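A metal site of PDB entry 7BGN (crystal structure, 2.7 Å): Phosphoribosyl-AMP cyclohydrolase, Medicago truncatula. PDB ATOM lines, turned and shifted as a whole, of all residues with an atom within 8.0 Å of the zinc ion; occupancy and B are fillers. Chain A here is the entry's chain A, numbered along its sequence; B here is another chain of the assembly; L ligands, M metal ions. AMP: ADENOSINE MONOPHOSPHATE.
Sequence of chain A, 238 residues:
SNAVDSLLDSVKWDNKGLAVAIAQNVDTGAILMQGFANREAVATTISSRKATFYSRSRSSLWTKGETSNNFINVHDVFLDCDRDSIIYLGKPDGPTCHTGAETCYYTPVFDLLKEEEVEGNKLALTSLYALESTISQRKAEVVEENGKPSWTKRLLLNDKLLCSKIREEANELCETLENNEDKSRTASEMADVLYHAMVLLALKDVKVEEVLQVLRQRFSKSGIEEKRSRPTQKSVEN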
ATOM      1  N   LYS A 165     -15.830  19.738 -14.007  1.00  0.00           N
ATOM      2  CA  LYS A 165     -16.877  20.450 -13.275  1.00  0.00           C
ATOM      3  C   LYS A 165     -17.921  19.484 -12.743  1.00  0.00           C
ATOM      4  O   LYS A 165     -18.374  19.610 -11.605  1.00  0.00           O
ATOM      5  CB  LYS A 165     -17.525  21.482 -14.194  1.00  0.00           C
ATOM      6  CG  LYS A 165     -17.878  22.843 -13.603  1.00  0.00           C
ATOM      7  CD  LYS A 165     -17.782  22.911 -12.096  1.00  0.00           C
ATOM      8  CE  LYS A 165     -18.379  24.213 -11.552  1.00  0.00           C
ATOM      9  NZ  LYS A 165     -17.885  24.449 -10.172  1.00  0.00           N
ATOM     10  N   GLU A 168     -16.290  17.489  -9.865  1.00  0.00           N
ATOM     11  CA  GLU A 168     -16.137  18.348  -8.688  1.00  0.00           C
ATOM     12  C   GLU A 168     -17.470  18.686  -8.042  1.00  0.00           C
ATOM     13  O   GLU A 168     -17.572  18.738  -6.813  1.00  0.00           O
ATOM     14  CB  GLU A 168     -15.350  19.597  -9.057  1.00  0.00           C
ATOM     15  CG  GLU A 168     -13.867  19.298  -9.201  1.00  0.00           C
ATOM     16  CD  GLU A 168     -13.247  18.750  -7.932  1.00  0.00           C
ATOM     17  OE1 GLU A 168     -12.307  17.928  -8.044  1.00  0.00           O
ATOM     18  OE2 GLU A 168     -13.717  19.106  -6.821  1.00  0.00           O
ATOM     19  N   GLU A 169     -18.508  18.978  -8.839  1.00  0.00           N
ATOM     20  CA  GLU A 169     -19.812  19.285  -8.252  1.00  0.00           C
ATOM     21  C   GLU A 169     -20.417  18.054  -7.596  1.00  0.00           C
ATOM     22  O   GLU A 169     -21.090  18.165  -6.557  1.00  0.00           O
ATOM     23  CB  GLU A 169     -20.770  19.851  -9.301  1.00  0.00           C
ATOM     24  CG  GLU A 169     -20.465  21.244  -9.802  1.00  0.00           C
ATOM     25  CD  GLU A 169     -20.679  22.327  -8.757  1.00  0.00           C
ATOM     26  OE1 GLU A 169     -20.994  21.998  -7.607  1.00  0.00           O
ATOM     27  OE2 GLU A 169     -20.578  23.524  -9.116  1.00  0.00           O
ATOM     28  N   ALA A 170     -20.218  16.869  -8.186  1.00  0.00           N
ATOM     29  CA  ALA A 170     -20.669  15.660  -7.519  1.00  0.00           C
ATOM     30  C   ALA A 170     -19.957  15.506  -6.176  1.00  0.00           C
ATOM     31  O   ALA A 170     -20.563  15.072  -5.192  1.00  0.00           O
ATOM     32  CB  ALA A 170     -20.405  14.448  -8.402  1.00  0.00           C
ATOM     33  N   ASN A 171     -18.678  15.885  -6.127  1.00  0.00           N
ATOM     34  CA  ASN A 171     -17.957  15.857  -4.871  1.00  0.00           C
ATOM     35  C   ASN A 171     -18.615  16.788  -3.854  1.00  0.00           C
ATOM     36  O   ASN A 171     -18.807  16.409  -2.702  1.00  0.00           O
ATOM     37  CB  ASN A 171     -16.492  16.219  -5.114  1.00  0.00           C
ATOM     38  CG  ASN A 171     -15.652  16.099  -3.866  1.00  0.00           C
ATOM     39  OD1 ASN A 171     -15.902  15.242  -3.031  1.00  0.00           O
ATOM     40  ND2 ASN A 171     -14.651  16.977  -3.740  1.00  0.00           N
ATOM     41  N   GLU A 172     -18.979  18.007  -4.279  1.00  0.00           N
ATOM     42  CA  GLU A 172     -19.589  18.974  -3.371  1.00  0.00           C
ATOM     43  C   GLU A 172     -20.952  18.515  -2.870  1.00  0.00           C
ATOM     44  O   GLU A 172     -21.320  18.802  -1.727  1.00  0.00           O
ATOM     45  CB  GLU A 172     -19.717  20.332  -4.040  1.00  0.00           C
ATOM     46  CG  GLU A 172     -18.460  21.151  -4.157  1.00  0.00           C
ATOM     47  CD  GLU A 172     -18.066  21.840  -2.861  1.00  0.00           C
ATOM     48  OE1 GLU A 172     -18.959  22.219  -2.058  1.00  0.00           O
ATOM     49  OE2 GLU A 172     -16.858  22.023  -2.668  1.00  0.00           O
ATOM     50  N   LEU A 173     -21.744  17.857  -3.719  1.00  0.00           N
ATOM     51  CA  LEU A 173     -23.039  17.336  -3.281  1.00  0.00           C
ATOM     52  C   LEU A 173     -22.868  16.345  -2.144  1.00  0.00           C
ATOM     53  O   LEU A 173     -23.608  16.400  -1.157  1.00  0.00           O
ATOM     54  CB  LEU A 173     -23.779  16.678  -4.451  1.00  0.00           C
ATOM     55  CG  LEU A 173     -25.121  16.012  -4.119  1.00  0.00           C
ATOM     56  CD1 LEU A 173     -26.188  17.039  -3.681  1.00  0.00           C
ATOM     57  CD2 LEU A 173     -25.614  15.190  -5.296  1.00  0.00           C
ATOM     58  N   THR A 176     -22.172  17.813   1.332  1.00  0.00           N
ATOM     59  CA  THR A 176     -23.317  18.272   2.124  1.00  0.00           C
ATOM     60  C   THR A 176     -23.849  17.163   3.014  1.00  0.00           C
ATOM     61  O   THR A 176     -24.345  17.424   4.113  1.00  0.00           O
ATOM     62  CB  THR A 176     -24.454  18.795   1.245  1.00  0.00           C
ATOM     63  OG1 THR A 176     -25.026  17.720   0.509  1.00  0.00           O
ATOM     64  CG2 THR A 176     -23.968  19.860   0.278  1.00  0.00           C
ATOM     65  N   ARG A 185     -28.393  23.543   1.352  1.00  0.00           N
ATOM     66  CA  ARG A 185     -27.081  23.372   0.731  1.00  0.00           C
ATOM     67  C   ARG A 185     -27.064  22.177  -0.210  1.00  0.00           C
ATOM     68  O   ARG A 185     -26.516  22.250  -1.320  1.00  0.00           O
ATOM     69  CB  ARG A 185     -26.007  23.213   1.812  1.00  0.00           C
ATOM     70  CG  ARG A 185     -25.730  24.465   2.629  1.00  0.00           C
ATOM     71  CD  ARG A 185     -25.154  25.489   1.724  1.00  0.00           C
ATOM     72  NE  ARG A 185     -24.066  24.867   1.011  1.00  0.00           N
ATOM     73  CZ  ARG A 185     -23.791  25.117  -0.256  1.00  0.00           C
ATOM     74  NH1 ARG A 185     -24.556  25.969  -0.934  1.00  0.00           N
ATOM     75  NH2 ARG A 185     -22.784  24.496  -0.849  1.00  0.00           N
ATOM     76  N   SER A 188     -29.001  23.030  -3.333  1.00  0.00           N
ATOM     77  CA  SER A 188     -28.222  23.957  -4.145  1.00  0.00           C
ATOM     78  C   SER A 188     -27.129  23.220  -4.909  1.00  0.00           C
ATOM     79  O   SER A 188     -26.847  23.538  -6.070  1.00  0.00           O
ATOM     80  CB  SER A 188     -27.642  25.049  -3.266  1.00  0.00           C
ATOM     81  OG  SER A 188     -26.883  25.955  -4.047  1.00  0.00           O
ATOM     82  N   GLU A 189     -26.483  22.244  -4.265  1.00  0.00           N
ATOM     83  CA  GLU A 189     -25.457  21.473  -4.951  1.00  0.00           C
ATOM     84  C   GLU A 189     -26.042  20.444  -5.918  1.00  0.00           C
ATOM     85  O   GLU A 189     -25.442  20.185  -6.967  1.00  0.00           O
ATOM     86  CB  GLU A 189     -24.551  20.778  -3.942  1.00  0.00           C
ATOM     87  CG  GLU A 189     -23.116  21.189  -4.096  1.00  0.00           C
ATOM     88  CD  GLU A 189     -22.852  22.653  -3.779  1.00  0.00           C
ATOM     89  OE1 GLU A 189     -22.244  23.355  -4.599  1.00  0.00           O
ATOM     90  OE2 GLU A 189     -23.240  23.098  -2.681  1.00  0.00           O
ATOM     91  N   MET A 190     -27.209  19.879  -5.606  1.00  0.00           N
ATOM     92  CA  MET A 190     -27.865  18.988  -6.562  1.00  0.00           C
ATOM     93  C   MET A 190     -28.210  19.733  -7.838  1.00  0.00           C
ATOM     94  O   MET A 190     -28.062  19.194  -8.944  1.00  0.00           O
ATOM     95  CB  MET A 190     -29.126  18.383  -5.942  1.00  0.00           C
ATOM     96  CG  MET A 190     -29.840  17.367  -6.833  1.00  0.00           C
ATOM     97  SD  MET A 190     -28.810  15.942  -7.252  1.00  0.00           S
ATOM     98  CE  MET A 190     -29.800  15.190  -8.525  1.00  0.00           C
ATOM     99  N   ALA A 191     -28.637  20.991  -7.701  1.00  0.00           N
ATOM    100  CA  ALA A 191     -28.849  21.834  -8.873  1.00  0.00           C
ATOM    101  C   ALA A 191     -27.543  22.051  -9.634  1.00  0.00           C
ATOM    102  O   ALA A 191     -27.539  22.080 -10.878  1.00  0.00           O
ATOM    103  CB  ALA A 191     -29.461  23.161  -8.439  1.00  0.00           C
ATOM    104  N   ASP A 192     -26.428  22.234  -8.915  1.00  0.00           N
ATOM    105  CA  ASP A 192     -25.122  22.362  -9.550  1.00  0.00           C
ATOM    106  C   ASP A 192     -24.757  21.101 -10.328  1.00  0.00           C
ATOM    107  O   ASP A 192     -24.149  21.183 -11.403  1.00  0.00           O
ATOM    108  CB  ASP A 192     -24.052  22.661  -8.515  1.00  0.00           C
ATOM    109  CG  ASP A 192     -24.183  24.039  -7.918  1.00  0.00           C
ATOM    110  OD1 ASP A 192     -25.136  24.759  -8.278  1.00  0.00           O
ATOM    111  OD2 ASP A 192     -23.309  24.404  -7.089  1.00  0.00           O
ATOM    112  N   VAL A 193     -25.028  19.928  -9.769  1.00  0.00           N
ATOM    113  CA  VAL A 193     -24.747  18.693 -10.501  1.00  0.00           C
ATOM    114  C   VAL A 193     -25.651  18.583 -11.718  1.00  0.00           C
ATOM    115  O   VAL A 193     -25.195  18.283 -12.830  1.00  0.00           O
ATOM    116  CB  VAL A 193     -24.906  17.481  -9.573  1.00  0.00           C
ATOM    117  CG1 VAL A 193     -24.841  16.206 -10.388  1.00  0.00           C
ATOM    118  CG2 VAL A 193     -23.852  17.499  -8.507  1.00  0.00           C
ATOM    119  N   HIS A 196     -24.707  20.997 -14.917  1.00  0.00           N
ATOM    120  CA  HIS A 196     -23.513  20.614 -15.657  1.00  0.00           C
ATOM    121  C   HIS A 196     -23.671  19.261 -16.343  1.00  0.00           C
ATOM    122  O   HIS A 196     -23.198  19.076 -17.467  1.00  0.00           O
ATOM    123  CB  HIS A 196     -22.313  20.606 -14.713  1.00  0.00           C
ATOM    124  CG  HIS A 196     -21.991  21.959 -14.168  1.00  0.00           C
ATOM    125  ND1 HIS A 196     -22.511  22.424 -12.982  1.00  0.00           N
ATOM    126  CD2 HIS A 196     -21.247  22.970 -14.678  1.00  0.00           C
ATOM    127  CE1 HIS A 196     -22.085  23.661 -12.769  1.00  0.00           C
ATOM    128  NE2 HIS A 196     -21.325  24.018 -13.786  1.00  0.00           N
ATOM    129  N   ARG B 218     -32.399  30.282 -11.000  1.00  0.00           N
ATOM    130  CA  ARG B 218     -31.141  30.707 -11.601  1.00  0.00           C
ATOM    131  C   ARG B 218     -31.277  31.112 -13.063  1.00  0.00           C
ATOM    132  O   ARG B 218     -30.273  31.322 -13.732  1.00  0.00           O
ATOM    133  CB  ARG B 218     -30.091  29.599 -11.495  1.00  0.00           C
ATOM    134  CG  ARG B 218     -29.699  29.253 -10.084  1.00  0.00           C
ATOM    135  CD  ARG B 218     -28.648  28.146 -10.054  1.00  0.00           C
ATOM    136  NE  ARG B 218     -28.431  27.671  -8.690  1.00  0.00           N
ATOM    137  CZ  ARG B 218     -27.693  26.605  -8.389  1.00  0.00           C
ATOM    138  NH1 ARG B 218     -27.094  25.914  -9.348  1.00  0.00           N
ATOM    139  NH2 ARG B 218     -27.567  26.240  -7.111  1.00  0.00           N
HETATM  140  P   AMP L   1     -25.729  31.001 -19.725  1.00  0.00           P
HETATM  141  O1P AMP L   1     -26.278  32.258 -20.345  1.00  0.00           O
HETATM  142  O2P AMP L   1     -25.420  29.891 -20.704  1.00  0.00           O
HETATM  143  O3P AMP L   1     -24.540  31.287 -18.802  1.00  0.00           O
HETATM  144  O5' AMP L   1     -26.864  30.430 -18.758  1.00  0.00           O
HETATM  145  C5' AMP L   1     -28.148  30.044 -19.239  1.00  0.00           C
HETATM  146  C4' AMP L   1     -28.937  29.326 -18.164  1.00  0.00           C
HETATM  147  O4' AMP L   1     -28.147  28.223 -17.669  1.00  0.00           O
HETATM  148  C3' AMP L   1     -29.241  30.137 -16.920  1.00  0.00           C
HETATM  149  O3' AMP L   1     -30.371  30.992 -17.069  1.00  0.00           O
HETATM  150  C2' AMP L   1     -29.405  29.078 -15.838  1.00  0.00           C
HETATM  151  O2' AMP L   1     -30.707  28.510 -15.860  1.00  0.00           O
HETATM  152  C1' AMP L   1     -28.413  28.010 -16.305  1.00  0.00           C
HETATM  153  N9  AMP L   1     -27.137  28.103 -15.583  1.00  0.00           N
HETATM  154  C8  AMP L   1     -26.016  28.781 -15.989  1.00  0.00           C
HETATM  155  N7  AMP L   1     -25.013  28.679 -15.160  1.00  0.00           N
HETATM  156  C5  AMP L   1     -25.510  27.899 -14.132  1.00  0.00           C
HETATM  157  C6  AMP L   1     -24.930  27.430 -12.936  1.00  0.00           C
HETATM  158  N6  AMP L   1     -23.680  27.713 -12.572  1.00  0.00           N
HETATM  159  N1  AMP L   1     -25.699  26.671 -12.125  1.00  0.00           N
HETATM  160  C2  AMP L   1     -26.956  26.390 -12.501  1.00  0.00           C
HETATM  161  N3  AMP L   1     -27.606  26.772 -13.607  1.00  0.00           N
HETATM  162  C4  AMP L   1     -26.818  27.530 -14.387  1.00  0.00           C
HETATM  163 ZN    ZN M   1     -21.771  23.305  -6.427  1.00  0.00          ZN
HETATM  164 MG    MG M   2     -18.523  23.156  -0.025  1.00  0.00          MG
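The zinc ion is bound by the side-chain carboxylate of Glu 189 (1.9 Å), the side-chain carboxylate of Glu 169 (1.9 Å) and the side-chain carboxylate of Asp 192 (2.0 Å).
The zinc ion has three donor atoms within binding distance.
Of the 17 residues printed, 3 come within 4 Å of the zinc ion.
Along chain A the residues within 4 Å of the zinc ion span positions 169 to 192.
The backbone carbonyl oxygen (O) of Arg 218 of chain B sits close to an oxygen (O3') of the ligand.
The guanidinium group (NH1) of Arg 218 of chain B sits close to a nitrogen (N1) of the ligand, at 3.2 Å.
OE2 of Glu 189 is in salt-bridge range of NH1 of Arg 185 (3.6 Å).
The side-chain carboxylate (OE2) of Glu 169 is in salt-bridge range of the side-chain amino group (NZ) of Lys 165, 3.0 Å away.
A ring nitrogen (ND1) of His 196 is in hydrogen-bond range of the backbone carbonyl oxygen (O) of Asp 192.
The side-chain carboxylate (OD1) of Asp 192 is in salt-bridge range of the guanidinium group (NH1) of Arg 218 of chain B (2.5 Å).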
